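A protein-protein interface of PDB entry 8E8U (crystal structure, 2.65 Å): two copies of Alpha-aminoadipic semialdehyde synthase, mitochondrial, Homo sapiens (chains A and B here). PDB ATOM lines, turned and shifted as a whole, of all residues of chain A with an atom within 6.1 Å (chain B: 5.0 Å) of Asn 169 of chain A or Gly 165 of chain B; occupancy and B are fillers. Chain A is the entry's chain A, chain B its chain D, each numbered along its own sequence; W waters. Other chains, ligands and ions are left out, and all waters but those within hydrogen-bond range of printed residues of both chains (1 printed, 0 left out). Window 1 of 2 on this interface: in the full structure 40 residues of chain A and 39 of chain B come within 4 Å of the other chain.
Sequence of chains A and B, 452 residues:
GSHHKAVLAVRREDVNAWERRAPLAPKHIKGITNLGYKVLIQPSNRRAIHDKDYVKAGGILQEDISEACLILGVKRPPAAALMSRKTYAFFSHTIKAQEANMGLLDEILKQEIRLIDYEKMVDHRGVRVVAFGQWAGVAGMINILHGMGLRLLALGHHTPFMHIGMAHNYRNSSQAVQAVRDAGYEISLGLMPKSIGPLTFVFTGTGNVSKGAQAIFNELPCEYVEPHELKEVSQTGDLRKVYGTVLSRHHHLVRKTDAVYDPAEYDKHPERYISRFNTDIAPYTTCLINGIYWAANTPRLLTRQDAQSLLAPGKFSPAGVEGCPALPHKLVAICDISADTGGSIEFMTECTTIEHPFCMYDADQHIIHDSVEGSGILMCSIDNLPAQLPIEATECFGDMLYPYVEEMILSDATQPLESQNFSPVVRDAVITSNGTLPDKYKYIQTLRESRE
Water W1 lies within hydrogen-bond range of the side-chain amide nitrogen (NE2) of Gln 175 of chain A (2.9 Å) and the backbone carbonyl oxygen (O) of His 163 of chain B (3.1 Å).
Of chain B, only His 146 (3.5 Å), Met 162 (3.5 Å), His 163 (3.1 Å), Ile 164 (3.8 Å) and Gly 165 (3.9 Å) come within 4 Å of Asn 169 of chain A.
Gly 165 of chain B touches one residue of chain A.
Printed residues of chain B within 4 Å of His 146 of chain A: Asn 169 (3.5 Å).
Of the printed residues of chain A, Asn 169 of chain B touches His 146 (3.5 Å).
Of the printed residues of chain A, His 163 of chain B touches Asn 169 (3.1 Å), Tyr 170 (3.7 Å) and Arg 171 (3.6 Å).
His 146 of chain A touches Asn 169 of chain B (CE1 to ND2, 3.5 Å).
His 146 of chain B touches Asn 169 of chain A.
CA of Asn 169 of chain A touches O of Met 162 of chain B, 3.5 Å away.
Ile 164 of chain B touches Asn 169 of chain A.
Gly 165 of chain B touches Asn 169 of chain A.
Tyr 170 of chain A touches His 163 of chain B (O to CD2, 3.7 Å).
His 163 of chain B touches Arg 171 of chain A.
His 146 of chain A touches Asn 169 of chain B, and with the chains exchanged Asn 169 of chain A touches His 146 of chain B.
Asn 169 of chain A touches Gly 165 of chain B, but with the chains exchanged Gly 165 of chain A does not touch Asn 169 of chain B (4.2 Å).
6 positions are printed for both chains.
Of the 9 pairs that touch across the chains among the printed residues, 2 have their exchanged pair printed and touching as well.
O of Met 162 of chain B lies close to O of His 168 of chain A (3.0 Å).
The backbone carbonyl oxygen of His 163 of chain B sits close to the backbone carbonyl oxygen of Asn 169 of chain A (3.1 Å).
The backbone NH (N) of Arg 171 of chain A is in hydrogen-bond range of the side-chain amide oxygen (OE1) of Gln 175 of chain A (2.8 Å).
O of Ile 164 of chain B is in hydrogen-bond range of ND1 of His 146 of chain B.
The backbone NH (N) of Gly 165 of chain B is in hydrogen-bond range of the side-chain hydroxyl (OH) of Tyr 170 of chain B (2.8 Å).
NE2 of Gln 388 of chain A is in hydrogen-bond range of ND1 of His 168 of chain A (3.3 Å).
The backbone NH of Gly 165 of chain A sits at hydrogen-bond distance from the side-chain hydroxyl of Tyr 170 of chain A (2.8 Å).
The backbone NH (N) of Met 166 of chain A lies close to the side-chain amide nitrogen (ND2) of Asn 169 of chain A (3.3 Å).
Of the 10 printed residues of chain B, 6 touch a printed residue of chain A.
Hydrophobic or aromatic side chains of chain B that line the printed part of chain A: His 146 and His 163.
Of the 10 printed residues of chain A, 5 touch a printed residue of chain B.
Hydrophobic or aromatic side chains of chain A that line the printed part of chain B: His 146.
Among the printed residues, no Asp or Glu carboxylate lies within 4 Å of a Lys or Arg side-chain nitrogen of the other chain.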
ATOM      1  N   HIS A 146      -6.810   1.630  -8.113  1.00  0.00           N
ATOM      2  CA  HIS A 146      -8.038   1.705  -8.897  1.00  0.00           C
ATOM      3  C   HIS A 146      -8.530   3.141  -9.006  1.00  0.00           C
ATOM      4  O   HIS A 146      -8.975   3.575 -10.075  1.00  0.00           O
ATOM      5  CB  HIS A 146      -9.105   0.808  -8.270  1.00  0.00           C
ATOM      6  CG  HIS A 146     -10.486   1.040  -8.801  1.00  0.00           C
ATOM      7  ND1 HIS A 146     -10.915   0.525 -10.006  1.00  0.00           N
ATOM      8  CD2 HIS A 146     -11.537   1.721  -8.287  1.00  0.00           C
ATOM      9  CE1 HIS A 146     -12.169   0.884 -10.213  1.00  0.00           C
ATOM     10  NE2 HIS A 146     -12.570   1.609  -9.185  1.00  0.00           N
ATOM     11  N   GLY A 165      -9.102  -3.364 -10.381  1.00  0.00           N
ATOM     12  CA  GLY A 165     -10.402  -3.144  -9.788  1.00  0.00           C
ATOM     13  C   GLY A 165     -10.328  -2.846  -8.302  1.00  0.00           C
ATOM     14  O   GLY A 165      -9.257  -2.697  -7.712  1.00  0.00           O
ATOM     15  N   MET A 166     -11.507  -2.752  -7.695  1.00  0.00           N
ATOM     16  CA  MET A 166     -11.602  -2.579  -6.255  1.00  0.00           C
ATOM     17  C   MET A 166     -11.211  -3.869  -5.538  1.00  0.00           C
ATOM     18  O   MET A 166     -11.248  -4.965  -6.106  1.00  0.00           O
ATOM     19  CB  MET A 166     -13.018  -2.165  -5.855  1.00  0.00           C
ATOM     20  CG  MET A 166     -13.409  -0.758  -6.286  1.00  0.00           C
ATOM     21  SD  MET A 166     -12.755   0.529  -5.201  1.00  0.00           S
ATOM     22  CE  MET A 166     -13.487   0.062  -3.636  1.00  0.00           C
ATOM     23  N   ALA A 167     -10.819  -3.720  -4.270  1.00  0.00           N
ATOM     24  CA  ALA A 167     -10.393  -4.873  -3.480  1.00  0.00           C
ATOM     25  C   ALA A 167     -11.494  -5.922  -3.382  1.00  0.00           C
ATOM     26  O   ALA A 167     -11.227  -7.126  -3.480  1.00  0.00           O
ATOM     27  CB  ALA A 167      -9.949  -4.424  -2.089  1.00  0.00           C
ATOM     28  N   HIS A 168     -12.743  -5.489  -3.188  1.00  0.00           N
ATOM     29  CA  HIS A 168     -13.838  -6.440  -3.039  1.00  0.00           C
ATOM     30  C   HIS A 168     -14.198  -7.141  -4.343  1.00  0.00           C
ATOM     31  O   HIS A 168     -15.004  -8.077  -4.316  1.00  0.00           O
ATOM     32  CB  HIS A 168     -15.074  -5.742  -2.466  1.00  0.00           C
ATOM     33  CG  HIS A 168     -15.607  -4.643  -3.332  1.00  0.00           C
ATOM     34  ND1 HIS A 168     -15.285  -3.317  -3.135  1.00  0.00           N
ATOM     35  CD2 HIS A 168     -16.449  -4.672  -4.392  1.00  0.00           C
ATOM     36  CE1 HIS A 168     -15.901  -2.577  -4.040  1.00  0.00           C
ATOM     37  NE2 HIS A 168     -16.613  -3.375  -4.815  1.00  0.00           N
ATOM     38  N   ASN A 169     -13.631  -6.717  -5.471  1.00  0.00           N
ATOM     39  CA  ASN A 169     -13.843  -7.403  -6.740  1.00  0.00           C
ATOM     40  C   ASN A 169     -12.952  -8.626  -6.909  1.00  0.00           C
ATOM     41  O   ASN A 169     -13.089  -9.337  -7.910  1.00  0.00           O
ATOM     42  CB  ASN A 169     -13.619  -6.445  -7.913  1.00  0.00           C
ATOM     43  CG  ASN A 169     -14.686  -5.374  -8.007  1.00  0.00           C
ATOM     44  OD1 ASN A 169     -15.830  -5.584  -7.601  1.00  0.00           O
ATOM     45  ND2 ASN A 169     -14.319  -4.220  -8.553  1.00  0.00           N
ATOM     46  N   TYR A 170     -12.042  -8.885  -5.975  1.00  0.00           N
ATOM     47  CA  TYR A 170     -11.112  -9.998  -6.081  1.00  0.00           C
ATOM     48  C   TYR A 170     -11.411 -11.043  -5.015  1.00  0.00           C
ATOM     49  O   TYR A 170     -11.772 -10.708  -3.882  1.00  0.00           O
ATOM     50  CB  TYR A 170      -9.662  -9.519  -5.959  1.00  0.00           C
ATOM     51  CG  TYR A 170      -9.245  -8.577  -7.065  1.00  0.00           C
ATOM     52  CD1 TYR A 170      -8.964  -9.056  -8.337  1.00  0.00           C
ATOM     53  CD2 TYR A 170      -9.133  -7.211  -6.840  1.00  0.00           C
ATOM     54  CE1 TYR A 170      -8.586  -8.203  -9.355  1.00  0.00           C
ATOM     55  CE2 TYR A 170      -8.754  -6.349  -7.853  1.00  0.00           C
ATOM     56  CZ  TYR A 170      -8.482  -6.852  -9.108  1.00  0.00           C
ATOM     57  OH  TYR A 170      -8.103  -6.000 -10.119  1.00  0.00           O
ATOM     58  N   ARG A 171     -11.266 -12.313  -5.401  1.00  0.00           N
ATOM     59  CA  ARG A 171     -11.524 -13.418  -4.483  1.00  0.00           C
ATOM     60  C   ARG A 171     -10.585 -13.380  -3.285  1.00  0.00           C
ATOM     61  O   ARG A 171     -11.000 -13.640  -2.150  1.00  0.00           O
ATOM     62  CB  ARG A 171     -11.392 -14.743  -5.229  1.00  0.00           C
ATOM     63  CG  ARG A 171     -11.601 -15.975  -4.372  1.00  0.00           C
ATOM     64  CD  ARG A 171     -11.365 -17.245  -5.177  1.00  0.00           C
ATOM     65  NE  ARG A 171      -9.963 -17.405  -5.556  1.00  0.00           N
ATOM     66  CZ  ARG A 171      -9.465 -17.076  -6.745  1.00  0.00           C
ATOM     67  NH1 ARG A 171     -10.255 -16.568  -7.682  1.00  0.00           N
ATOM     68  NH2 ARG A 171      -8.176 -17.257  -6.998  1.00  0.00           N
ATOM     69  N   GLN A 175      -5.328 -13.084  -6.264  1.00  0.00           N
ATOM     70  CA  GLN A 175      -5.928 -12.665  -7.526  1.00  0.00           C
ATOM     71  C   GLN A 175      -5.724 -11.175  -7.769  1.00  0.00           C
ATOM     72  O   GLN A 175      -5.561 -10.749  -8.917  1.00  0.00           O
ATOM     73  CB  GLN A 175      -7.418 -13.014  -7.541  1.00  0.00           C
ATOM     74  CG  GLN A 175      -8.063 -12.919  -8.915  1.00  0.00           C
ATOM     75  CD  GLN A 175      -9.563 -13.140  -8.878  1.00  0.00           C
ATOM     76  OE1 GLN A 175     -10.235 -12.767  -7.916  1.00  0.00           O
ATOM     77  NE2 GLN A 175     -10.096 -13.746  -9.931  1.00  0.00           N
ATOM     78  N   GLN A 388     -13.141  -5.891   2.716  1.00  0.00           N
ATOM     79  CA  GLN A 388     -13.015  -6.137   1.285  1.00  0.00           C
ATOM     80  C   GLN A 388     -12.259  -7.427   0.988  1.00  0.00           C
ATOM     81  O   GLN A 388     -12.441  -8.004  -0.089  1.00  0.00           O
ATOM     82  CB  GLN A 388     -12.317  -4.955   0.615  1.00  0.00           C
ATOM     83  CG  GLN A 388     -13.086  -3.650   0.711  1.00  0.00           C
ATOM     84  CD  GLN A 388     -12.407  -2.521  -0.033  1.00  0.00           C
ATOM     85  OE1 GLN A 388     -11.516  -1.860   0.498  1.00  0.00           O
ATOM     86  NE2 GLN A 388     -12.824  -2.293  -1.273  1.00  0.00           N
ATOM     87  N   ILE B 142     -20.323  -9.013 -18.620  1.00  0.00           N
ATOM     88  CA  ILE B 142     -19.417  -8.792 -17.496  1.00  0.00           C
ATOM     89  C   ILE B 142     -20.054  -7.850 -16.483  1.00  0.00           C
ATOM     90  O   ILE B 142     -20.007  -8.087 -15.269  1.00  0.00           O
ATOM     91  CB  ILE B 142     -18.064  -8.254 -17.994  1.00  0.00           C
ATOM     92  CG1 ILE B 142     -17.431  -9.234 -18.982  1.00  0.00           C
ATOM     93  CG2 ILE B 142     -17.128  -8.001 -16.823  1.00  0.00           C
ATOM     94  CD1 ILE B 142     -16.373  -8.608 -19.858  1.00  0.00           C
ATOM     95  N   HIS B 146     -21.268  -8.700 -12.629  1.00  0.00           N
ATOM     96  CA  HIS B 146     -20.793  -7.856 -11.539  1.00  0.00           C
ATOM     97  C   HIS B 146     -21.958  -7.244 -10.768  1.00  0.00           C
ATOM     98  O   HIS B 146     -21.938  -7.199  -9.533  1.00  0.00           O
ATOM     99  CB  HIS B 146     -19.875  -6.768 -12.094  1.00  0.00           C
ATOM    100  CG  HIS B 146     -19.590  -5.660 -11.128  1.00  0.00           C
ATOM    101  ND1 HIS B 146     -18.669  -5.777 -10.111  1.00  0.00           N
ATOM    102  CD2 HIS B 146     -20.099  -4.410 -11.033  1.00  0.00           C
ATOM    103  CE1 HIS B 146     -18.626  -4.649  -9.426  1.00  0.00           C
ATOM    104  NE2 HIS B 146     -19.484  -3.802  -9.966  1.00  0.00           N
ATOM    105  N   MET B 162     -19.465 -11.715  -6.680  1.00  0.00           N
ATOM    106  CA  MET B 162     -18.769 -10.599  -6.049  1.00  0.00           C
ATOM    107  C   MET B 162     -17.336 -10.460  -6.545  1.00  0.00           C
ATOM    108  O   MET B 162     -16.744  -9.383  -6.410  1.00  0.00           O
ATOM    109  CB  MET B 162     -18.764 -10.772  -4.531  1.00  0.00           C
ATOM    110  CG  MET B 162     -20.064 -10.403  -3.844  1.00  0.00           C
ATOM    111  SD  MET B 162     -20.381  -8.633  -3.922  1.00  0.00           S
ATOM    112  CE  MET B 162     -18.870  -7.995  -3.201  1.00  0.00           C
ATOM    113  N   HIS B 163     -16.768 -11.521  -7.118  1.00  0.00           N
ATOM    114  CA  HIS B 163     -15.383 -11.529  -7.561  1.00  0.00           C
ATOM    115  C   HIS B 163     -15.246 -11.255  -9.054  1.00  0.00           C
ATOM    116  O   HIS B 163     -14.226 -11.609  -9.654  1.00  0.00           O
ATOM    117  CB  HIS B 163     -14.736 -12.862  -7.188  1.00  0.00           C
ATOM    118  CG  HIS B 163     -14.911 -13.225  -5.746  1.00  0.00           C
ATOM    119  ND1 HIS B 163     -15.082 -14.523  -5.318  1.00  0.00           N
ATOM    120  CD2 HIS B 163     -14.950 -12.454  -4.634  1.00  0.00           C
ATOM    121  CE1 HIS B 163     -15.216 -14.536  -4.003  1.00  0.00           C
ATOM    122  NE2 HIS B 163     -15.138 -13.293  -3.564  1.00  0.00           N
ATOM    123  N   ILE B 164     -16.252 -10.634  -9.663  1.00  0.00           N
ATOM    124  CA  ILE B 164     -16.193 -10.175 -11.046  1.00  0.00           C
ATOM    125  C   ILE B 164     -16.397  -8.667 -11.044  1.00  0.00           C
ATOM    126  O   ILE B 164     -17.416  -8.176 -10.542  1.00  0.00           O
ATOM    127  CB  ILE B 164     -17.242 -10.869 -11.929  1.00  0.00           C
ATOM    128  CG1 ILE B 164     -17.064 -12.388 -11.885  1.00  0.00           C
ATOM    129  CG2 ILE B 164     -17.155 -10.356 -13.359  1.00  0.00           C
ATOM    130  CD1 ILE B 164     -18.156 -13.150 -12.606  1.00  0.00           C
ATOM    131  N   GLY B 165     -15.430  -7.935 -11.592  1.00  0.00           N
ATOM    132  CA  GLY B 165     -15.497  -6.492 -11.655  1.00  0.00           C
ATOM    133  C   GLY B 165     -16.248  -6.002 -12.879  1.00  0.00           C
ATOM    134  O   GLY B 165     -16.822  -6.773 -13.651  1.00  0.00           O
ATOM    135  N   MET B 166     -16.237  -4.682 -13.052  1.00  0.00           N
ATOM    136  CA  MET B 166     -16.829  -4.080 -14.235  1.00  0.00           C
ATOM    137  C   MET B 166     -15.978  -4.378 -15.466  1.00  0.00           C
ATOM    138  O   MET B 166     -14.789  -4.696 -15.372  1.00  0.00           O
ATOM    139  CB  MET B 166     -16.986  -2.569 -14.052  1.00  0.00           C
ATOM    140  CG  MET B 166     -18.050  -2.172 -13.038  1.00  0.00           C
ATOM    141  SD  MET B 166     -19.726  -2.248 -13.710  1.00  0.00           S
ATOM    142  CE  MET B 166     -19.606  -1.087 -15.069  1.00  0.00           C
ATOM    143  N   ALA B 167     -16.615  -4.283 -16.637  1.00  0.00           N
ATOM    144  CA  ALA B 167     -15.927  -4.590 -17.889  1.00  0.00           C
ATOM    145  C   ALA B 167     -14.690  -3.720 -18.080  1.00  0.00           C
ATOM    146  O   ALA B 167     -13.641  -4.208 -18.516  1.00  0.00           O
ATOM    147  CB  ALA B 167     -16.886  -4.427 -19.068  1.00  0.00           C
ATOM    148  N   ASN B 169     -12.746  -2.611 -15.939  1.00  0.00           N
ATOM    149  CA  ASN B 169     -11.700  -2.948 -14.981  1.00  0.00           C
ATOM    150  C   ASN B 169     -10.716  -3.988 -15.505  1.00  0.00           C
ATOM    151  O   ASN B 169      -9.739  -4.292 -14.812  1.00  0.00           O
ATOM    152  CB  ASN B 169     -12.320  -3.452 -13.675  1.00  0.00           C
ATOM    153  CG  ASN B 169     -13.064  -2.365 -12.922  1.00  0.00           C
ATOM    154  OD1 ASN B 169     -14.086  -2.622 -12.285  1.00  0.00           O
ATOM    155  ND2 ASN B 169     -12.551  -1.141 -12.990  1.00  0.00           N
ATOM    156  N   TYR B 170     -10.944  -4.538 -16.695  1.00  0.00           N
ATOM    157  CA  TYR B 170     -10.102  -5.586 -17.255  1.00  0.00           C
ATOM    158  C   TYR B 170      -9.357  -5.062 -18.474  1.00  0.00           C
ATOM    159  O   TYR B 170      -9.891  -4.255 -19.242  1.00  0.00           O
ATOM    160  CB  TYR B 170     -10.935  -6.814 -17.627  1.00  0.00           C
ATOM    161  CG  TYR B 170     -11.624  -7.452 -16.441  1.00  0.00           C
ATOM    162  CD1 TYR B 170     -10.913  -8.231 -15.537  1.00  0.00           C
ATOM    163  CD2 TYR B 170     -12.984  -7.271 -16.221  1.00  0.00           C
ATOM    164  CE1 TYR B 170     -11.536  -8.812 -14.448  1.00  0.00           C
ATOM    165  CE2 TYR B 170     -13.616  -7.850 -15.136  1.00  0.00           C
ATOM    166  CZ  TYR B 170     -12.888  -8.619 -14.254  1.00  0.00           C
ATOM    167  OH  TYR B 170     -13.514  -9.196 -13.172  1.00  0.00           O
HETATM  168  O   HOH W   1     -12.924 -14.244 -10.543  1.00  0.00           O
